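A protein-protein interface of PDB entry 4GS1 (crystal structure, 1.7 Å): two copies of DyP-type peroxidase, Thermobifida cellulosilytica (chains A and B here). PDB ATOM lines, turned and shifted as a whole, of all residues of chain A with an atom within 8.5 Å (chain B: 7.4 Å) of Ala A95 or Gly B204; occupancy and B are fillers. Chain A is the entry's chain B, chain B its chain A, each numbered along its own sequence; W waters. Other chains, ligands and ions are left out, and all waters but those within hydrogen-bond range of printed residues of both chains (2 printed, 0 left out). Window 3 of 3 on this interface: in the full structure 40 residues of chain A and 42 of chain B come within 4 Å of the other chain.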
ATOM      1  N   PRO A  92      -0.842  -9.764 -29.573  1.00  0.00           N
ATOM      2  CA  PRO A  92      -0.693  -9.855 -28.113  1.00  0.00           C
ATOM      3  C   PRO A  92       0.593  -9.230 -27.576  1.00  0.00           C
ATOM      4  O   PRO A  92       1.614  -9.229 -28.266  1.00  0.00           O
ATOM      5  CB  PRO A  92      -0.684 -11.368 -27.856  1.00  0.00           C
ATOM      6  CG  PRO A  92      -1.423 -11.958 -29.054  1.00  0.00           C
ATOM      7  CD  PRO A  92      -0.978 -11.089 -30.202  1.00  0.00           C
ATOM      8  N   GLU A  93       0.528  -8.737 -26.340  1.00  0.00           N
ATOM      9  CA  GLU A  93       1.646  -8.073 -25.666  1.00  0.00           C
ATOM     10  C   GLU A  93       2.803  -9.011 -25.303  1.00  0.00           C
ATOM     11  O   GLU A  93       3.974  -8.654 -25.456  1.00  0.00           O
ATOM     12  CB  GLU A  93       1.127  -7.372 -24.396  1.00  0.00           C
ATOM     13  CG  GLU A  93       2.140  -6.489 -23.661  1.00  0.00           C
ATOM     14  CD  GLU A  93       3.092  -7.269 -22.763  1.00  0.00           C
ATOM     15  OE1 GLU A  93       2.646  -8.224 -22.087  1.00  0.00           O
ATOM     16  OE2 GLU A  93       4.295  -6.928 -22.738  1.00  0.00           O
ATOM     17  N   GLY A  94       2.476 -10.204 -24.820  1.00  0.00           N
ATOM     18  CA  GLY A  94       3.471 -11.069 -24.199  1.00  0.00           C
ATOM     19  C   GLY A  94       4.706 -11.456 -24.999  1.00  0.00           C
ATOM     20  O   GLY A  94       4.775 -11.245 -26.210  1.00  0.00           O
ATOM     21  N   ALA A  95       5.694 -12.028 -24.314  1.00  0.00           N
ATOM     22  CA  ALA A  95       6.842 -12.612 -24.994  1.00  0.00           C
ATOM     23  C   ALA A  95       6.426 -13.926 -25.639  1.00  0.00           C
ATOM     24  O   ALA A  95       7.067 -14.390 -26.579  1.00  0.00           O
ATOM     25  CB  ALA A  95       7.999 -12.832 -24.024  1.00  0.00           C
ATOM     26  N   ALA A  96       5.352 -14.523 -25.133  1.00  0.00           N
ATOM     27  CA  ALA A  96       4.875 -15.812 -25.638  1.00  0.00           C
ATOM     28  C   ALA A  96       4.543 -15.772 -27.131  1.00  0.00           C
ATOM     29  O   ALA A  96       4.714 -16.772 -27.836  1.00  0.00           O
ATOM     30  CB  ALA A  96       3.671 -16.284 -24.841  1.00  0.00           C
ATOM     31  N   SER A  97       4.062 -14.626 -27.605  1.00  0.00           N
ATOM     32  CA  SER A  97       3.716 -14.485 -29.020  1.00  0.00           C
ATOM     33  C   SER A  97       4.760 -13.702 -29.824  1.00  0.00           C
ATOM     34  O   SER A  97       4.505 -13.311 -30.964  1.00  0.00           O
ATOM     35  CB  SER A  97       2.332 -13.850 -29.183  1.00  0.00           C
ATOM     36  OG  SER A  97       2.282 -12.582 -28.570  1.00  0.00           O
ATOM     37  N   ALA A  98       5.939 -13.484 -29.245  1.00  0.00           N
ATOM     38  CA  ALA A  98       7.012 -12.798 -29.968  1.00  0.00           C
ATOM     39  C   ALA A  98       7.428 -13.574 -31.220  1.00  0.00           C
ATOM     40  O   ALA A  98       7.480 -14.810 -31.207  1.00  0.00           O
ATOM     41  CB  ALA A  98       8.211 -12.576 -29.055  1.00  0.00           C
ATOM     42  N   GLY A  99       7.720 -12.848 -32.299  1.00  0.00           N
ATOM     43  CA  GLY A  99       8.194 -13.467 -33.526  1.00  0.00           C
ATOM     44  C   GLY A  99       7.122 -14.168 -34.339  1.00  0.00           C
ATOM     45  O   GLY A  99       7.440 -14.931 -35.258  1.00  0.00           O
ATOM     46  N   LEU A 100       5.857 -13.925 -34.005  1.00  0.00           N
ATOM     47  CA  LEU A 100       4.747 -14.528 -34.743  1.00  0.00           C
ATOM     48  C   LEU A 100       4.016 -13.511 -35.610  1.00  0.00           C
ATOM     49  O   LEU A 100       3.973 -12.316 -35.293  1.00  0.00           O
ATOM     50  CB  LEU A 100       3.752 -15.184 -33.781  1.00  0.00           C
ATOM     51  CG  LEU A 100       4.361 -16.192 -32.812  1.00  0.00           C
ATOM     52  CD1 LEU A 100       3.265 -16.853 -31.974  1.00  0.00           C
ATOM     53  CD2 LEU A 100       5.159 -17.220 -33.576  1.00  0.00           C
ATOM     54  N   MET A 159      -0.585 -20.513 -30.739  1.00  0.00           N
ATOM     55  CA  MET A 159       0.193 -19.734 -29.775  1.00  0.00           C
ATOM     56  C   MET A 159      -0.259 -18.271 -29.760  1.00  0.00           C
ATOM     57  O   MET A 159      -0.379 -17.657 -28.691  1.00  0.00           O
ATOM     58  CB  MET A 159       1.691 -19.860 -30.072  1.00  0.00           C
ATOM     59  CG  MET A 159       2.567 -19.228 -29.036  1.00  0.00           C
ATOM     60  SD  MET A 159       2.328 -19.993 -27.423  1.00  0.00           S
ATOM     61  CE  MET A 159       4.029 -19.969 -26.851  1.00  0.00           C
ATOM     62  N   ALA A 163      -2.019 -16.672 -26.297  1.00  0.00           N
ATOM     63  CA  ALA A 163      -1.514 -15.428 -25.734  1.00  0.00           C
ATOM     64  C   ALA A 163      -2.630 -14.396 -25.628  1.00  0.00           C
ATOM     65  O   ALA A 163      -2.737 -13.698 -24.622  1.00  0.00           O
ATOM     66  CB  ALA A 163      -0.352 -14.892 -26.568  1.00  0.00           C
ATOM     67  N   PRO B 199      11.181 -22.440 -30.656  1.00  0.00           N
ATOM     68  CA  PRO B 199       9.836 -22.120 -30.159  1.00  0.00           C
ATOM     69  C   PRO B 199       9.847 -21.618 -28.729  1.00  0.00           C
ATOM     70  O   PRO B 199      10.786 -21.900 -27.977  1.00  0.00           O
ATOM     71  CB  PRO B 199       9.120 -23.475 -30.196  1.00  0.00           C
ATOM     72  CG  PRO B 199       9.888 -24.294 -31.206  1.00  0.00           C
ATOM     73  CD  PRO B 199      11.316 -23.862 -31.018  1.00  0.00           C
ATOM     74  N   ARG B 200       8.801 -20.886 -28.357  1.00  0.00           N
ATOM     75  CA  ARG B 200       8.625 -20.415 -26.984  1.00  0.00           C
ATOM     76  C   ARG B 200       7.519 -21.169 -26.250  1.00  0.00           C
ATOM     77  O   ARG B 200       6.647 -21.785 -26.876  1.00  0.00           O
ATOM     78  CB  ARG B 200       8.311 -18.913 -26.978  1.00  0.00           C
ATOM     79  CG  ARG B 200       9.468 -18.048 -27.452  1.00  0.00           C
ATOM     80  CD  ARG B 200       9.050 -16.582 -27.594  1.00  0.00           C
ATOM     81  NE  ARG B 200      10.136 -15.735 -28.099  1.00  0.00           N
ATOM     82  CZ  ARG B 200      10.941 -15.002 -27.336  1.00  0.00           C
ATOM     83  NH1 ARG B 200      10.799 -14.991 -26.016  1.00  0.00           N
ATOM     84  NH2 ARG B 200      11.899 -14.276 -27.898  1.00  0.00           N
ATOM     85  N   ASN B 201       7.546 -21.110 -24.922  1.00  0.00           N
ATOM     86  CA  ASN B 201       6.511 -21.743 -24.102  1.00  0.00           C
ATOM     87  C   ASN B 201       5.510 -20.712 -23.575  1.00  0.00           C
ATOM     88  O   ASN B 201       5.615 -19.524 -23.897  1.00  0.00           O
ATOM     89  CB  ASN B 201       7.148 -22.566 -22.961  1.00  0.00           C
ATOM     90  CG  ASN B 201       7.925 -21.714 -21.974  1.00  0.00           C
ATOM     91  OD1 ASN B 201       7.584 -20.560 -21.733  1.00  0.00           O
ATOM     92  ND2 ASN B 201       8.974 -22.292 -21.378  1.00  0.00           N
ATOM     93  N   LEU B 202       4.551 -21.150 -22.755  1.00  0.00           N
ATOM     94  CA  LEU B 202       3.464 -20.260 -22.341  1.00  0.00           C
ATOM     95  C   LEU B 202       3.904 -19.215 -21.316  1.00  0.00           C
ATOM     96  O   LEU B 202       3.183 -18.247 -21.060  1.00  0.00           O
ATOM     97  CB  LEU B 202       2.252 -21.055 -21.820  1.00  0.00           C
ATOM     98  CG  LEU B 202       1.503 -21.890 -22.860  1.00  0.00           C
ATOM     99  CD1 LEU B 202       0.475 -22.813 -22.215  1.00  0.00           C
ATOM    100  CD2 LEU B 202       0.820 -20.974 -23.857  1.00  0.00           C
ATOM    101  N   MET B 203       5.091 -19.398 -20.740  1.00  0.00           N
ATOM    102  CA  MET B 203       5.668 -18.373 -19.870  1.00  0.00           C
ATOM    103  C   MET B 203       6.409 -17.319 -20.679  1.00  0.00           C
ATOM    104  O   MET B 203       6.926 -16.349 -20.123  1.00  0.00           O
ATOM    105  CB  MET B 203       6.621 -19.007 -18.861  1.00  0.00           C
ATOM    106  CG  MET B 203       5.929 -19.557 -17.625  1.00  0.00           C
ATOM    107  SD  MET B 203       7.069 -20.525 -16.616  1.00  0.00           S
ATOM    108  CE  MET B 203       6.113 -20.652 -15.109  1.00  0.00           C
ATOM    109  N   GLY B 204       6.465 -17.513 -21.991  1.00  0.00           N
ATOM    110  CA  GLY B 204       7.136 -16.571 -22.873  1.00  0.00           C
ATOM    111  C   GLY B 204       8.587 -16.914 -23.167  1.00  0.00           C
ATOM    112  O   GLY B 204       9.249 -16.222 -23.938  1.00  0.00           O
ATOM    113  N   GLN B 205       9.092 -17.980 -22.556  1.00  0.00           N
ATOM    114  CA  GLN B 205      10.518 -18.295 -22.645  1.00  0.00           C
ATOM    115  C   GLN B 205      10.881 -19.070 -23.903  1.00  0.00           C
ATOM    116  O   GLN B 205      10.166 -19.989 -24.300  1.00  0.00           O
ATOM    117  CB  GLN B 205      10.927 -19.130 -21.432  1.00  0.00           C
ATOM    118  CG  GLN B 205      10.748 -18.413 -20.105  1.00  0.00           C
ATOM    119  CD  GLN B 205      10.311 -19.346 -18.994  1.00  0.00           C
ATOM    120  OE1 GLN B 205      10.075 -20.539 -19.215  1.00  0.00           O
ATOM    121  NE2 GLN B 205      10.177 -18.801 -17.794  1.00  0.00           N
ATOM    122  N   ILE B 206      12.007 -18.718 -24.517  1.00  0.00           N
ATOM    123  CA  ILE B 206      12.574 -19.555 -25.562  1.00  0.00           C
ATOM    124  C   ILE B 206      12.956 -20.880 -24.905  1.00  0.00           C
ATOM    125  O   ILE B 206      13.589 -20.895 -23.846  1.00  0.00           O
ATOM    126  CB  ILE B 206      13.797 -18.869 -26.221  1.00  0.00           C
ATOM    127  CG1 ILE B 206      13.327 -17.692 -27.089  1.00  0.00           C
ATOM    128  CG2 ILE B 206      14.581 -19.868 -27.059  1.00  0.00           C
ATOM    129  CD1 ILE B 206      14.445 -16.727 -27.518  1.00  0.00           C
ATOM    130  N   ASP B 207      12.548 -21.991 -25.511  1.00  0.00           N
ATOM    131  CA  ASP B 207      12.650 -23.303 -24.859  1.00  0.00           C
ATOM    132  C   ASP B 207      13.247 -24.328 -25.819  1.00  0.00           C
ATOM    133  O   ASP B 207      12.604 -24.714 -26.807  1.00  0.00           O
ATOM    134  CB  ASP B 207      11.250 -23.755 -24.395  1.00  0.00           C
ATOM    135  CG  ASP B 207      11.292 -24.756 -23.253  1.00  0.00           C
ATOM    136  OD1 ASP B 207      12.307 -25.481 -23.138  1.00  0.00           O
ATOM    137  OD2 ASP B 207      10.304 -24.822 -22.468  1.00  0.00           O
ATOM    138  N   MET B 249       1.671 -24.814 -15.318  1.00  0.00           N
ATOM    139  CA  MET B 249       2.324 -23.541 -15.027  1.00  0.00           C
ATOM    140  C   MET B 249       1.396 -22.652 -14.230  1.00  0.00           C
ATOM    141  O   MET B 249       0.229 -22.493 -14.587  1.00  0.00           O
ATOM    142  CB  MET B 249       2.699 -22.817 -16.326  1.00  0.00           C
ATOM    143  CG  MET B 249       3.837 -23.459 -17.083  1.00  0.00           C
ATOM    144  SD  MET B 249       3.931 -22.729 -18.740  1.00  0.00           S
ATOM    145  CE  MET B 249       5.580 -23.229 -19.243  1.00  0.00           C
ATOM    146  N   LEU B 251       0.436 -19.624 -14.043  1.00  0.00           N
ATOM    147  CA  LEU B 251       0.557 -18.432 -14.874  1.00  0.00           C
ATOM    148  C   LEU B 251       0.040 -17.173 -14.188  1.00  0.00           C
ATOM    149  O   LEU B 251       0.547 -16.083 -14.439  1.00  0.00           O
ATOM    150  CB  LEU B 251      -0.136 -18.638 -16.226  1.00  0.00           C
ATOM    151  CG  LEU B 251       0.517 -19.642 -17.179  1.00  0.00           C
ATOM    152  CD1 LEU B 251      -0.363 -19.855 -18.412  1.00  0.00           C
ATOM    153  CD2 LEU B 251       1.896 -19.178 -17.609  1.00  0.00           C
ATOM    154  N   TRP B 254       2.864 -16.112 -12.084  1.00  0.00           N
ATOM    155  CA  TRP B 254       3.923 -15.687 -12.991  1.00  0.00           C
ATOM    156  C   TRP B 254       3.704 -14.250 -13.472  1.00  0.00           C
ATOM    157  O   TRP B 254       4.651 -13.478 -13.590  1.00  0.00           O
ATOM    158  CB  TRP B 254       3.974 -16.651 -14.185  1.00  0.00           C
ATOM    159  CG  TRP B 254       5.077 -16.401 -15.197  1.00  0.00           C
ATOM    160  CD1 TRP B 254       4.929 -15.960 -16.485  1.00  0.00           C
ATOM    161  CD2 TRP B 254       6.486 -16.607 -15.005  1.00  0.00           C
ATOM    162  NE1 TRP B 254       6.157 -15.882 -17.103  1.00  0.00           N
ATOM    163  CE2 TRP B 254       7.129 -16.270 -16.215  1.00  0.00           C
ATOM    164  CE3 TRP B 254       7.264 -17.047 -13.928  1.00  0.00           C
ATOM    165  CZ2 TRP B 254       8.520 -16.354 -16.379  1.00  0.00           C
ATOM    166  CZ3 TRP B 254       8.643 -17.130 -14.089  1.00  0.00           C
ATOM    167  CH2 TRP B 254       9.256 -16.783 -15.302  1.00  0.00           C
ATOM    168  N   VAL B 259       9.539  -8.194 -15.731  1.00  0.00           N
ATOM    169  CA  VAL B 259      10.408  -8.939 -16.649  1.00  0.00           C
ATOM    170  C   VAL B 259      11.767  -9.349 -16.042  1.00  0.00           C
ATOM    171  O   VAL B 259      12.156 -10.511 -16.160  1.00  0.00           O
ATOM    172  CB  VAL B 259      10.560  -8.236 -18.033  1.00  0.00           C
ATOM    173  CG1 VAL B 259      11.695  -8.855 -18.838  1.00  0.00           C
ATOM    174  CG2 VAL B 259       9.253  -8.315 -18.809  1.00  0.00           C
ATOM    175  N   ARG B 262      11.328 -12.318 -13.800  1.00  0.00           N
ATOM    176  CA  ARG B 262      11.058 -13.521 -14.592  1.00  0.00           C
ATOM    177  C   ARG B 262      12.355 -14.080 -15.151  1.00  0.00           C
ATOM    178  O   ARG B 262      12.578 -15.295 -15.148  1.00  0.00           O
ATOM    179  CB  ARG B 262      10.102 -13.219 -15.753  1.00  0.00           C
ATOM    180  CG  ARG B 262       8.690 -12.929 -15.311  1.00  0.00           C
ATOM    181  CD  ARG B 262       7.764 -12.674 -16.485  1.00  0.00           C
ATOM    182  NE  ARG B 262       6.591 -11.924 -16.039  1.00  0.00           N
ATOM    183  CZ  ARG B 262       5.530 -11.661 -16.791  1.00  0.00           C
ATOM    184  NH1 ARG B 262       5.473 -12.106 -18.041  1.00  0.00           N
ATOM    185  NH2 ARG B 262       4.521 -10.959 -16.280  1.00  0.00           N
ATOM    186  N   HIS B 269      17.614 -14.107 -20.716  1.00  0.00           N
ATOM    187  CA  HIS B 269      16.737 -13.006 -21.110  1.00  0.00           C
ATOM    188  C   HIS B 269      15.496 -13.497 -21.839  1.00  0.00           C
ATOM    189  O   HIS B 269      15.547 -14.480 -22.575  1.00  0.00           O
ATOM    190  CB  HIS B 269      17.479 -12.029 -22.018  1.00  0.00           C
ATOM    191  CG  HIS B 269      18.491 -11.191 -21.304  1.00  0.00           C
ATOM    192  ND1 HIS B 269      18.151 -10.061 -20.593  1.00  0.00           N
ATOM    193  CD2 HIS B 269      19.835 -11.315 -21.197  1.00  0.00           C
ATOM    194  CE1 HIS B 269      19.245  -9.522 -20.077  1.00  0.00           C
ATOM    195  NE2 HIS B 269      20.279 -10.266 -20.430  1.00  0.00           N
ATOM    196  N   LEU B 270      14.376 -12.808 -21.645  1.00  0.00           N
ATOM    197  CA  LEU B 270      13.151 -13.187 -22.341  1.00  0.00           C
ATOM    198  C   LEU B 270      13.160 -12.762 -23.804  1.00  0.00           C
ATOM    199  O   LEU B 270      12.735 -13.522 -24.674  1.00  0.00           O
ATOM    200  CB  LEU B 270      11.921 -12.612 -21.638  1.00  0.00           C
ATOM    201  CG  LEU B 270      11.377 -13.450 -20.484  1.00  0.00           C
ATOM    202  CD1 LEU B 270      10.387 -12.641 -19.664  1.00  0.00           C
ATOM    203  CD2 LEU B 270      10.735 -14.733 -20.996  1.00  0.00           C
ATOM    204  N   ASP B 271      13.637 -11.551 -24.081  1.00  0.00           N
ATOM    205  CA  ASP B 271      13.603 -11.049 -25.455  1.00  0.00           C
ATOM    206  C   ASP B 271      14.535 -11.811 -26.405  1.00  0.00           C
ATOM    207  O   ASP B 271      14.103 -12.283 -27.461  1.00  0.00           O
ATOM    208  CB  ASP B 271      13.838  -9.526 -25.513  1.00  0.00           C
ATOM    209  CG  ASP B 271      15.121  -9.090 -24.822  1.00  0.00           C
ATOM    210  OD1 ASP B 271      15.779  -9.920 -24.157  1.00  0.00           O
ATOM    211  OD2 ASP B 271      15.470  -7.893 -24.937  1.00  0.00           O
HETATM  212  O   HOH W   1       4.961  -9.277 -19.759  1.00  0.00           O
HETATM  213  O   HOH W   2      10.382 -16.034 -30.991  1.00  0.00           O
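The guanidinium group of Arg B200 lies within hydrogen-bond range of the backbone carbonyl oxygen of Gly B204 (2.9 Å). The backbone carbonyl oxygen (O) of Leu B270 lies within hydrogen-bond range of the guanidinium group (NH1) of Arg B200. The side-chain amide oxygen of Asn B201 is in hydrogen-bond range of the backbone NH of Met B203 (2.9 Å). N of Gly B204 lies within hydrogen-bond range of OD1 of Asn B201, 3.3 Å away. OE1 of Gln B205 sits at hydrogen-bond distance from ND2 of Asn B201. ND2 of Asn B201 lies within hydrogen-bond range of OD2 of Asp B207 (3.1 Å).
O of Ala A95 touches CD of Arg B200, 3.1 Å away. Ala A95 touches Gly B204 (CB to O, 3.6 Å). O of Asn B201 touches CB of Ala A96, 3.9 Å away. Ala A96 touches Gly B204 (N to CA, 3.5 Å). Ala A98 touches Arg B200 (CB to NE, 3.8 Å). Met A159 touches Arg B200 (CE to O, 3.2 Å). Asn B201 touches Met A159. Met A159 touches Leu B202.
Ala A95 touches just these residues of chain B: Arg B200 and Gly B204. Of the printed residues of chain A, Gly B204 touches Ala A95 (3.6 Å) and Ala A96 (3.5 Å). Of the printed residues of chain B, Ala A98 touches Arg B200 (3.8 Å). Of the printed residues of chain A, Leu B202 touches Met A159. Gly A94 touches none of the printed residues of chain B. Gly A99 touches none of the printed residues of chain B. The nearest printed residue of chain A that does not touch Gly B204 is Met A159 (6.0 Å).
Hydrophobic or aromatic side chains of chain A that line the printed part of chain B: Ala A95, Ala A96, Ala A98 and Met A159. Of the 17 printed residues of chain B, 4 touch a printed residue of chain A. Printed residues of chain B that touch a printed residue of chain A: Arg B200, Asn B201, Leu B202 and Gly B204. Hydrophobic or aromatic side chains of chain B within 4 Å of the printed part of chain A: Leu B202. Among the printed residues, no Asp or Glu carboxylate lies within 4 Å of a Lys or Arg side-chain nitrogen of the other chain.
No position is printed for both chains.
Water W2 lies within hydrogen-bond range of the guanidinium group of Arg B200 (2.9 Å) and the backbone carbonyl oxygen of Ala A98 (3.2 Å). Water W1 bridges the guanidinium group of Arg B262 (3.3 Å) and the side-chain carboxylate of Glu A93 (3.4 Å).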
